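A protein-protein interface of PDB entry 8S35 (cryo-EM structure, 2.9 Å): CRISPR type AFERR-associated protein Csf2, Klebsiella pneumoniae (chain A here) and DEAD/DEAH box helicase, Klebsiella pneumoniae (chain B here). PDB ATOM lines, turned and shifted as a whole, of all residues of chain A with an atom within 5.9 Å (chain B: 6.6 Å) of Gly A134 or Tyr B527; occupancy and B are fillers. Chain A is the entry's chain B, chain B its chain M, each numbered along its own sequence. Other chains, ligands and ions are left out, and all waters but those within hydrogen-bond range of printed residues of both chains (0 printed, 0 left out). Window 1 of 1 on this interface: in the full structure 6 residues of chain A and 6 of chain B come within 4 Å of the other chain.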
ATOM      1  N   LYS A   9     -11.737  -2.343  19.110  1.00  0.00           N
ATOM      2  CA  LYS A   9     -13.124  -2.744  19.253  1.00  0.00           C
ATOM      3  C   LYS A   9     -13.940  -1.618  19.863  1.00  0.00           C
ATOM      4  O   LYS A   9     -13.494  -0.937  20.794  1.00  0.00           O
ATOM      5  CB  LYS A   9     -13.248  -3.992  20.124  1.00  0.00           C
ATOM      6  CG  LYS A   9     -13.164  -5.288  19.349  1.00  0.00           C
ATOM      7  CD  LYS A   9     -13.372  -6.479  20.261  1.00  0.00           C
ATOM      8  CE  LYS A   9     -12.285  -7.516  20.064  1.00  0.00           C
ATOM      9  NZ  LYS A   9     -12.273  -8.047  18.674  1.00  0.00           N
ATOM     10  N   PRO A 132     -19.779  -6.210  13.405  1.00  0.00           N
ATOM     11  CA  PRO A 132     -20.034  -6.811  14.717  1.00  0.00           C
ATOM     12  C   PRO A 132     -19.284  -8.125  14.894  1.00  0.00           C
ATOM     13  O   PRO A 132     -18.749  -8.708  13.950  1.00  0.00           O
ATOM     14  CB  PRO A 132     -21.549  -7.047  14.731  1.00  0.00           C
ATOM     15  CG  PRO A 132     -22.058  -6.584  13.419  1.00  0.00           C
ATOM     16  CD  PRO A 132     -20.906  -6.461  12.493  1.00  0.00           C
ATOM     17  N   ASP A 133     -19.255  -8.578  16.143  1.00  0.00           N
ATOM     18  CA  ASP A 133     -18.665  -9.853  16.526  1.00  0.00           C
ATOM     19  C   ASP A 133     -19.766 -10.787  17.005  1.00  0.00           C
ATOM     20  O   ASP A 133     -20.573 -10.412  17.860  1.00  0.00           O
ATOM     21  CB  ASP A 133     -17.618  -9.661  17.624  1.00  0.00           C
ATOM     22  CG  ASP A 133     -16.579  -8.622  17.262  1.00  0.00           C
ATOM     23  OD1 ASP A 133     -16.573  -8.171  16.098  1.00  0.00           O
ATOM     24  OD2 ASP A 133     -15.767  -8.260  18.138  1.00  0.00           O
ATOM     25  N   GLY A 134     -19.797 -11.997  16.460  1.00  0.00           N
ATOM     26  CA  GLY A 134     -20.774 -12.997  16.851  1.00  0.00           C
ATOM     27  C   GLY A 134     -21.965 -13.045  15.912  1.00  0.00           C
ATOM     28  O   GLY A 134     -22.065 -12.312  14.924  1.00  0.00           O
ATOM     29  N   ASP A 135     -22.894 -13.942  16.253  1.00  0.00           N
ATOM     30  CA  ASP A 135     -24.020 -14.223  15.368  1.00  0.00           C
ATOM     31  C   ASP A 135     -25.123 -13.184  15.499  1.00  0.00           C
ATOM     32  O   ASP A 135     -25.613 -12.667  14.490  1.00  0.00           O
ATOM     33  CB  ASP A 135     -24.579 -15.617  15.660  1.00  0.00           C
ATOM     34  CG  ASP A 135     -25.540 -16.094  14.590  1.00  0.00           C
ATOM     35  OD1 ASP A 135     -25.178 -16.037  13.396  1.00  0.00           O
ATOM     36  OD2 ASP A 135     -26.658 -16.526  14.941  1.00  0.00           O
ATOM     37  N   ASN A 136     -25.538 -12.876  16.725  1.00  0.00           N
ATOM     38  CA  ASN A 136     -26.613 -11.923  16.972  1.00  0.00           C
ATOM     39  C   ASN A 136     -26.089 -10.817  17.874  1.00  0.00           C
ATOM     40  O   ASN A 136     -25.811 -11.051  19.056  1.00  0.00           O
ATOM     41  CB  ASN A 136     -27.818 -12.617  17.604  1.00  0.00           C
ATOM     42  CG  ASN A 136     -29.098 -11.825  17.443  1.00  0.00           C
ATOM     43  OD1 ASN A 136     -29.693 -11.379  18.423  1.00  0.00           O
ATOM     44  ND2 ASN A 136     -29.532 -11.648  16.201  1.00  0.00           N
ATOM     45  N   GLN A 137     -25.951  -9.618  17.311  1.00  0.00           N
ATOM     46  CA  GLN A 137     -25.635  -8.431  18.093  1.00  0.00           C
ATOM     47  C   GLN A 137     -26.469  -7.238  17.639  1.00  0.00           C
ATOM     48  O   GLN A 137     -26.072  -6.090  17.867  1.00  0.00           O
ATOM     49  CB  GLN A 137     -24.137  -8.117  18.019  1.00  0.00           C
ATOM     50  CG  GLN A 137     -23.298  -8.995  18.937  1.00  0.00           C
ATOM     51  CD  GLN A 137     -21.971  -8.368  19.310  1.00  0.00           C
ATOM     52  OE1 GLN A 137     -21.579  -7.336  18.769  1.00  0.00           O
ATOM     53  NE2 GLN A 137     -21.268  -8.997  20.244  1.00  0.00           N
ATOM     54  N   TRP A 138     -27.615  -7.480  17.007  1.00  0.00           N
ATOM     55  CA  TRP A 138     -28.484  -6.419  16.528  1.00  0.00           C
ATOM     56  C   TRP A 138     -29.932  -6.837  16.713  1.00  0.00           C
ATOM     57  O   TRP A 138     -30.247  -8.018  16.871  1.00  0.00           O
ATOM     58  CB  TRP A 138     -28.219  -6.096  15.056  1.00  0.00           C
ATOM     59  CG  TRP A 138     -28.280  -7.297  14.186  1.00  0.00           C
ATOM     60  CD1 TRP A 138     -29.375  -7.788  13.545  1.00  0.00           C
ATOM     61  CD2 TRP A 138     -27.198  -8.173  13.865  1.00  0.00           C
ATOM     62  NE1 TRP A 138     -29.042  -8.917  12.838  1.00  0.00           N
ATOM     63  CE2 TRP A 138     -27.710  -9.175  13.020  1.00  0.00           C
ATOM     64  CE3 TRP A 138     -25.844  -8.205  14.207  1.00  0.00           C
ATOM     65  CZ2 TRP A 138     -26.915 -10.197  12.511  1.00  0.00           C
ATOM     66  CZ3 TRP A 138     -25.059  -9.222  13.705  1.00  0.00           C
ATOM     67  CH2 TRP A 138     -25.596 -10.201  12.863  1.00  0.00           C
ATOM     68  N   GLU A 247     -19.878  -5.915  20.624  1.00  0.00           N
ATOM     69  CA  GLU A 247     -18.488  -5.676  20.262  1.00  0.00           C
ATOM     70  C   GLU A 247     -18.403  -5.571  18.746  1.00  0.00           C
ATOM     71  O   GLU A 247     -18.806  -6.499  18.037  1.00  0.00           O
ATOM     72  CB  GLU A 247     -17.596  -6.807  20.771  1.00  0.00           C
ATOM     73  CG  GLU A 247     -17.449  -6.854  22.285  1.00  0.00           C
ATOM     74  CD  GLU A 247     -16.444  -5.852  22.821  1.00  0.00           C
ATOM     75  OE1 GLU A 247     -15.690  -5.263  22.018  1.00  0.00           O
ATOM     76  OE2 GLU A 247     -16.409  -5.649  24.052  1.00  0.00           O
ATOM     77  N   SER A 249     -15.631  -4.919  15.809  1.00  0.00           N
ATOM     78  CA  SER A 249     -14.242  -4.730  15.423  1.00  0.00           C
ATOM     79  C   SER A 249     -14.147  -3.542  14.480  1.00  0.00           C
ATOM     80  O   SER A 249     -14.905  -3.446  13.510  1.00  0.00           O
ATOM     81  CB  SER A 249     -13.696  -5.988  14.753  1.00  0.00           C
ATOM     82  OG  SER A 249     -14.448  -6.312  13.598  1.00  0.00           O
ATOM     83  N   MET B 521     -23.046 -22.350  16.588  1.00  0.00           N
ATOM     84  CA  MET B 521     -22.135 -22.332  17.724  1.00  0.00           C
ATOM     85  C   MET B 521     -20.747 -22.828  17.351  1.00  0.00           C
ATOM     86  O   MET B 521     -19.754 -22.299  17.860  1.00  0.00           O
ATOM     87  CB  MET B 521     -22.724 -23.165  18.877  1.00  0.00           C
ATOM     88  CG  MET B 521     -21.743 -23.754  19.907  1.00  0.00           C
ATOM     89  SD  MET B 521     -20.753 -25.190  19.432  1.00  0.00           S
ATOM     90  CE  MET B 521     -19.885 -25.494  20.964  1.00  0.00           C
ATOM     91  N   LYS B 522     -20.650 -23.838  16.480  1.00  0.00           N
ATOM     92  CA  LYS B 522     -19.345 -24.213  15.944  1.00  0.00           C
ATOM     93  C   LYS B 522     -18.697 -23.023  15.256  1.00  0.00           C
ATOM     94  O   LYS B 522     -17.488 -22.799  15.384  1.00  0.00           O
ATOM     95  CB  LYS B 522     -19.489 -25.381  14.969  1.00  0.00           C
ATOM     96  CG  LYS B 522     -18.166 -26.030  14.586  1.00  0.00           C
ATOM     97  CD  LYS B 522     -18.350 -27.078  13.500  1.00  0.00           C
ATOM     98  CE  LYS B 522     -17.117 -27.958  13.362  1.00  0.00           C
ATOM     99  NZ  LYS B 522     -17.328 -29.077  12.405  1.00  0.00           N
ATOM    100  N   ALA B 523     -19.498 -22.234  14.538  1.00  0.00           N
ATOM    101  CA  ALA B 523     -18.996 -20.991  13.974  1.00  0.00           C
ATOM    102  C   ALA B 523     -18.567 -20.037  15.076  1.00  0.00           C
ATOM    103  O   ALA B 523     -17.510 -19.408  14.984  1.00  0.00           O
ATOM    104  CB  ALA B 523     -20.059 -20.343  13.091  1.00  0.00           C
ATOM    105  N   GLU B 524     -19.368 -19.934  16.136  1.00  0.00           N
ATOM    106  CA  GLU B 524     -19.019 -19.045  17.237  1.00  0.00           C
ATOM    107  C   GLU B 524     -17.748 -19.527  17.918  1.00  0.00           C
ATOM    108  O   GLU B 524     -16.883 -18.720  18.274  1.00  0.00           O
ATOM    109  CB  GLU B 524     -20.220 -18.931  18.198  1.00  0.00           C
ATOM    110  CG  GLU B 524     -20.088 -18.142  19.545  1.00  0.00           C
ATOM    111  CD  GLU B 524     -19.086 -18.669  20.575  1.00  0.00           C
ATOM    112  OE1 GLU B 524     -18.871 -17.960  21.578  1.00  0.00           O
ATOM    113  OE2 GLU B 524     -18.618 -19.821  20.473  1.00  0.00           O
ATOM    114  N   SER B 525     -17.626 -20.837  18.139  1.00  0.00           N
ATOM    115  CA  SER B 525     -16.437 -21.355  18.805  1.00  0.00           C
ATOM    116  C   SER B 525     -15.191 -21.126  17.959  1.00  0.00           C
ATOM    117  O   SER B 525     -14.147 -20.715  18.479  1.00  0.00           O
ATOM    118  CB  SER B 525     -16.617 -22.841  19.104  1.00  0.00           C
ATOM    119  OG  SER B 525     -15.794 -23.243  20.185  1.00  0.00           O
ATOM    120  N   LEU B 526     -15.284 -21.372  16.651  1.00  0.00           N
ATOM    121  CA  LEU B 526     -14.137 -21.128  15.783  1.00  0.00           C
ATOM    122  C   LEU B 526     -13.797 -19.644  15.732  1.00  0.00           C
ATOM    123  O   LEU B 526     -12.617 -19.273  15.710  1.00  0.00           O
ATOM    124  CB  LEU B 526     -14.418 -21.665  14.378  1.00  0.00           C
ATOM    125  CG  LEU B 526     -13.347 -21.409  13.310  1.00  0.00           C
ATOM    126  CD1 LEU B 526     -11.962 -21.829  13.782  1.00  0.00           C
ATOM    127  CD2 LEU B 526     -13.708 -22.132  12.024  1.00  0.00           C
ATOM    128  N   TYR B 527     -14.814 -18.781  15.704  1.00  0.00           N
ATOM    129  CA  TYR B 527     -14.565 -17.346  15.701  1.00  0.00           C
ATOM    130  C   TYR B 527     -13.871 -16.913  16.982  1.00  0.00           C
ATOM    131  O   TYR B 527     -12.936 -16.111  16.946  1.00  0.00           O
ATOM    132  CB  TYR B 527     -15.877 -16.586  15.518  1.00  0.00           C
ATOM    133  CG  TYR B 527     -15.731 -15.081  15.569  1.00  0.00           C
ATOM    134  CD1 TYR B 527     -14.650 -14.447  14.973  1.00  0.00           C
ATOM    135  CD2 TYR B 527     -16.676 -14.296  16.213  1.00  0.00           C
ATOM    136  CE1 TYR B 527     -14.513 -13.079  15.018  1.00  0.00           C
ATOM    137  CE2 TYR B 527     -16.547 -12.924  16.261  1.00  0.00           C
ATOM    138  CZ  TYR B 527     -15.464 -12.321  15.660  1.00  0.00           C
ATOM    139  OH  TYR B 527     -15.327 -10.954  15.703  1.00  0.00           O
ATOM    140  N   GLY B 528     -14.319 -17.431  18.125  1.00  0.00           N
ATOM    141  CA  GLY B 528     -13.659 -17.111  19.380  1.00  0.00           C
ATOM    142  C   GLY B 528     -12.225 -17.601  19.407  1.00  0.00           C
ATOM    143  O   GLY B 528     -11.328 -16.905  19.889  1.00  0.00           O
ATOM    144  N   TYR B 529     -11.993 -18.804  18.884  1.00  0.00           N
ATOM    145  CA  TYR B 529     -10.640 -19.346  18.826  1.00  0.00           C
ATOM    146  C   TYR B 529      -9.736 -18.451  17.990  1.00  0.00           C
ATOM    147  O   TYR B 529      -8.647 -18.063  18.428  1.00  0.00           O
ATOM    148  CB  TYR B 529     -10.682 -20.764  18.259  1.00  0.00           C
ATOM    149  CG  TYR B 529      -9.339 -21.303  17.827  1.00  0.00           C
ATOM    150  CD1 TYR B 529      -8.458 -21.846  18.751  1.00  0.00           C
ATOM    151  CD2 TYR B 529      -8.956 -21.279  16.492  1.00  0.00           C
ATOM    152  CE1 TYR B 529      -7.232 -22.343  18.360  1.00  0.00           C
ATOM    153  CE2 TYR B 529      -7.731 -21.772  16.092  1.00  0.00           C
ATOM    154  CZ  TYR B 529      -6.873 -22.304  17.029  1.00  0.00           C
ATOM    155  OH  TYR B 529      -5.650 -22.797  16.635  1.00  0.00           O
ATOM    156  N   LEU B 530     -10.178 -18.105  16.780  1.00  0.00           N
ATOM    157  CA  LEU B 530      -9.365 -17.263  15.908  1.00  0.00           C
ATOM    158  C   LEU B 530      -9.177 -15.871  16.502  1.00  0.00           C
ATOM    159  O   LEU B 530      -8.103 -15.272  16.372  1.00  0.00           O
ATOM    160  CB  LEU B 530     -10.012 -17.173  14.527  1.00  0.00           C
ATOM    161  CG  LEU B 530     -10.062 -18.487  13.747  1.00  0.00           C
ATOM    162  CD1 LEU B 530     -11.211 -18.479  12.756  1.00  0.00           C
ATOM    163  CD2 LEU B 530      -8.741 -18.737  13.036  1.00  0.00           C
ATOM    164  N   LYS B 531     -10.212 -15.342  17.157  1.00  0.00           N
ATOM    165  CA  LYS B 531     -10.114 -14.036  17.794  1.00  0.00           C
ATOM    166  C   LYS B 531      -9.072 -14.043  18.903  1.00  0.00           C
ATOM    167  O   LYS B 531      -8.280 -13.104  19.030  1.00  0.00           O
ATOM    168  CB  LYS B 531     -11.484 -13.637  18.340  1.00  0.00           C
ATOM    169  CG  LYS B 531     -11.552 -12.258  18.960  1.00  0.00           C
ATOM    170  CD  LYS B 531     -13.002 -11.827  19.127  1.00  0.00           C
ATOM    171  CE  LYS B 531     -13.220 -11.040  20.407  1.00  0.00           C
ATOM    172  NZ  LYS B 531     -14.346 -10.074  20.276  1.00  0.00           N
ATOM    173  N   GLU B 532      -9.056 -15.101  19.716  1.00  0.00           N
ATOM    174  CA  GLU B 532      -8.055 -15.196  20.771  1.00  0.00           C
ATOM    175  C   GLU B 532      -6.680 -15.506  20.198  1.00  0.00           C
ATOM    176  O   GLU B 532      -5.664 -15.116  20.782  1.00  0.00           O
ATOM    177  CB  GLU B 532      -8.461 -16.262  21.788  1.00  0.00           C
ATOM    178  CG  GLU B 532      -9.744 -15.942  22.543  1.00  0.00           C
ATOM    179  CD  GLU B 532      -9.594 -14.763  23.484  1.00  0.00           C
ATOM    180  OE1 GLU B 532      -8.449 -14.317  23.708  1.00  0.00           O
ATOM    181  OE2 GLU B 532     -10.623 -14.280  24.001  1.00  0.00           O
ATOM    182  N   TYR B 535      -6.055 -13.768  14.937  1.00  0.00           N
ATOM    183  CA  TYR B 535      -6.532 -13.648  13.567  1.00  0.00           C
ATOM    184  C   TYR B 535      -7.746 -12.732  13.513  1.00  0.00           C
ATOM    185  O   TYR B 535      -8.677 -12.864  14.314  1.00  0.00           O
ATOM    186  CB  TYR B 535      -6.880 -15.027  13.010  1.00  0.00           C
ATOM    187  CG  TYR B 535      -5.697 -15.962  12.930  1.00  0.00           C
ATOM    188  CD1 TYR B 535      -4.637 -15.700  12.074  1.00  0.00           C
ATOM    189  CD2 TYR B 535      -5.639 -17.105  13.714  1.00  0.00           C
ATOM    190  CE1 TYR B 535      -3.553 -16.551  11.999  1.00  0.00           C
ATOM    191  CE2 TYR B 535      -4.560 -17.963  13.646  1.00  0.00           C
ATOM    192  CZ  TYR B 535      -3.519 -17.681  12.788  1.00  0.00           C
ATOM    193  OH  TYR B 535      -2.441 -18.532  12.716  1.00  0.00           O
ATOM    194  N   SER B 536      -7.732 -11.802  12.564  1.00  0.00           N
ATOM    195  CA  SER B 536      -8.797 -10.816  12.396  1.00  0.00           C
ATOM    196  C   SER B 536      -9.692 -11.265  11.249  1.00  0.00           C
ATOM    197  O   SER B 536      -9.389 -11.021  10.079  1.00  0.00           O
ATOM    198  CB  SER B 536      -8.211  -9.434  12.133  1.00  0.00           C
ATOM    199  OG  SER B 536      -7.254  -9.481  11.091  1.00  0.00           O
ATOM    200  N   ARG B 537     -10.800 -11.920  11.585  1.00  0.00           N
ATOM    201  CA  ARG B 537     -11.764 -12.378  10.595  1.00  0.00           C
ATOM    202  C   ARG B 537     -13.161 -12.125  11.129  1.00  0.00           C
ATOM    203  O   ARG B 537     -13.443 -12.417  12.294  1.00  0.00           O
ATOM    204  CB  ARG B 537     -11.574 -13.865  10.282  1.00  0.00           C
ATOM    205  CG  ARG B 537     -10.208 -14.199   9.706  1.00  0.00           C
ATOM    206  CD  ARG B 537     -10.083 -15.677   9.368  1.00  0.00           C
ATOM    207  NE  ARG B 537     -11.052 -16.101   8.365  1.00  0.00           N
ATOM    208  CZ  ARG B 537     -11.005 -15.774   7.080  1.00  0.00           C
ATOM    209  NH1 ARG B 537     -10.038 -15.014   6.591  1.00  0.00           N
ATOM    210  NH2 ARG B 537     -11.953 -16.223   6.262  1.00  0.00           N
ATOM    211  N   THR B 538     -14.031 -11.590  10.280  1.00  0.00           N
ATOM    212  CA  THR B 538     -15.387 -11.291  10.704  1.00  0.00           C
ATOM    213  C   THR B 538     -16.143 -12.581  10.998  1.00  0.00           C
ATOM    214  O   THR B 538     -15.745 -13.675  10.592  1.00  0.00           O
ATOM    215  CB  THR B 538     -16.130 -10.497   9.631  1.00  0.00           C
ATOM    216  OG1 THR B 538     -16.310 -11.314   8.468  1.00  0.00           O
ATOM    217  CG2 THR B 538     -15.353  -9.247   9.257  1.00  0.00           C
ATOM    218  N   PHE B 539     -17.255 -12.440  11.721  1.00  0.00           N
ATOM    219  CA  PHE B 539     -18.063 -13.610  12.036  1.00  0.00           C
ATOM    220  C   PHE B 539     -18.616 -14.246  10.771  1.00  0.00           C
ATOM    221  O   PHE B 539     -18.687 -15.474  10.666  1.00  0.00           O
ATOM    222  CB  PHE B 539     -19.204 -13.242  12.980  1.00  0.00           C
ATOM    223  CG  PHE B 539     -20.045 -14.418  13.378  1.00  0.00           C
ATOM    224  CD1 PHE B 539     -19.666 -15.228  14.432  1.00  0.00           C
ATOM    225  CD2 PHE B 539     -21.202 -14.728  12.685  1.00  0.00           C
ATOM    226  CE1 PHE B 539     -20.430 -16.317  14.797  1.00  0.00           C
ATOM    227  CE2 PHE B 539     -21.968 -15.818  13.043  1.00  0.00           C
ATOM    228  CZ  PHE B 539     -21.582 -16.613  14.101  1.00  0.00           C
ATOM    229  N   GLU B 540     -19.027 -13.427   9.803  1.00  0.00           N
ATOM    230  CA  GLU B 540     -19.576 -13.985   8.575  1.00  0.00           C
ATOM    231  C   GLU B 540     -18.515 -14.732   7.780  1.00  0.00           C
ATOM    232  O   GLU B 540     -18.833 -15.704   7.089  1.00  0.00           O
ATOM    233  CB  GLU B 540     -20.196 -12.879   7.724  1.00  0.00           C
ATOM    234  CG  GLU B 540     -21.458 -12.273   8.321  1.00  0.00           C
ATOM    235  CD  GLU B 540     -22.603 -13.267   8.406  1.00  0.00           C
ATOM    236  OE1 GLU B 540     -22.590 -14.257   7.645  1.00  0.00           O
ATOM    237  OE2 GLU B 540     -23.513 -13.058   9.234  1.00  0.00           O
ATOM    238  N   VAL B 542     -16.134 -16.535   9.168  1.00  0.00           N
ATOM    239  CA  VAL B 542     -16.083 -17.836   9.821  1.00  0.00           C
ATOM    240  C   VAL B 542     -17.311 -18.657   9.458  1.00  0.00           C
ATOM    241  O   VAL B 542     -17.234 -19.881   9.313  1.00  0.00           O
ATOM    242  CB  VAL B 542     -15.948 -17.661  11.345  1.00  0.00           C
ATOM    243  CG1 VAL B 542     -15.853 -19.019  12.036  1.00  0.00           C
ATOM    244  CG2 VAL B 542     -14.734 -16.795  11.672  1.00  0.00           C
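Of the 10 printed residues of chain A, 4 touch a printed residue of chain B. Along chain B the printed residues that touch a printed residue of chain A span positions 527 to 539. Among the printed residues, 6 pairs touch across the chains. Among the printed residues, Asp or Glu carboxylates within 4 Å of a Lys or Arg side-chain nitrogen of the other chain: Asp A133 with Lys B531.
The side-chain carboxylate (OD2) of Asp A133 lies within salt-bridge range of the side-chain amino group (NZ) of Lys A9, 3.5 Å away. NE2 of Gln A137 sits at hydrogen-bond distance from O of Asp A133, 2.9 Å away. N of Asp A133 sits at hydrogen-bond distance from O of Glu A247 (2.8 Å). The side-chain carboxylate (OD1) of Asp A133 sits at hydrogen-bond distance from the backbone NH (N) of Ser A249 (3.4 Å).
Tyr B527 touches Gly A134. Gly A134 touches Phe B539. Asp A135 touches Phe B539 (OD1 to CE2, 3.2 Å).
OD1 of Asp A133 lies close to OH of Tyr B527, at 3.1 Å. NZ of Lys B531 lies within salt-bridge range of OD2 of Asp A133 (3.1 Å). The side-chain amino group (NZ) of Lys A9 lies close to the side-chain amino group (NZ) of Lys B531 (3.3 Å).
Printed residues of chain B within 4 Å of Lys A9: Lys B531 (3.3 Å). Gly A134 touches just these residues of chain B: Tyr B527 and Phe B539. Of chain A, only Asp A133 and Gly A134 come within 4 Å of Tyr B527. Of the printed residues of chain A, Lys B531 touches Lys A9 (3.3 Å) and Asp A133 (3.1 Å). Printed residues of chain A within 4 Å of Phe B539: Gly A134 (3.3 Å) and Asp A135 (3.2 Å). The nearest printed residue of chain A that does not touch Lys B531 is Glu A247 (4.6 Å).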
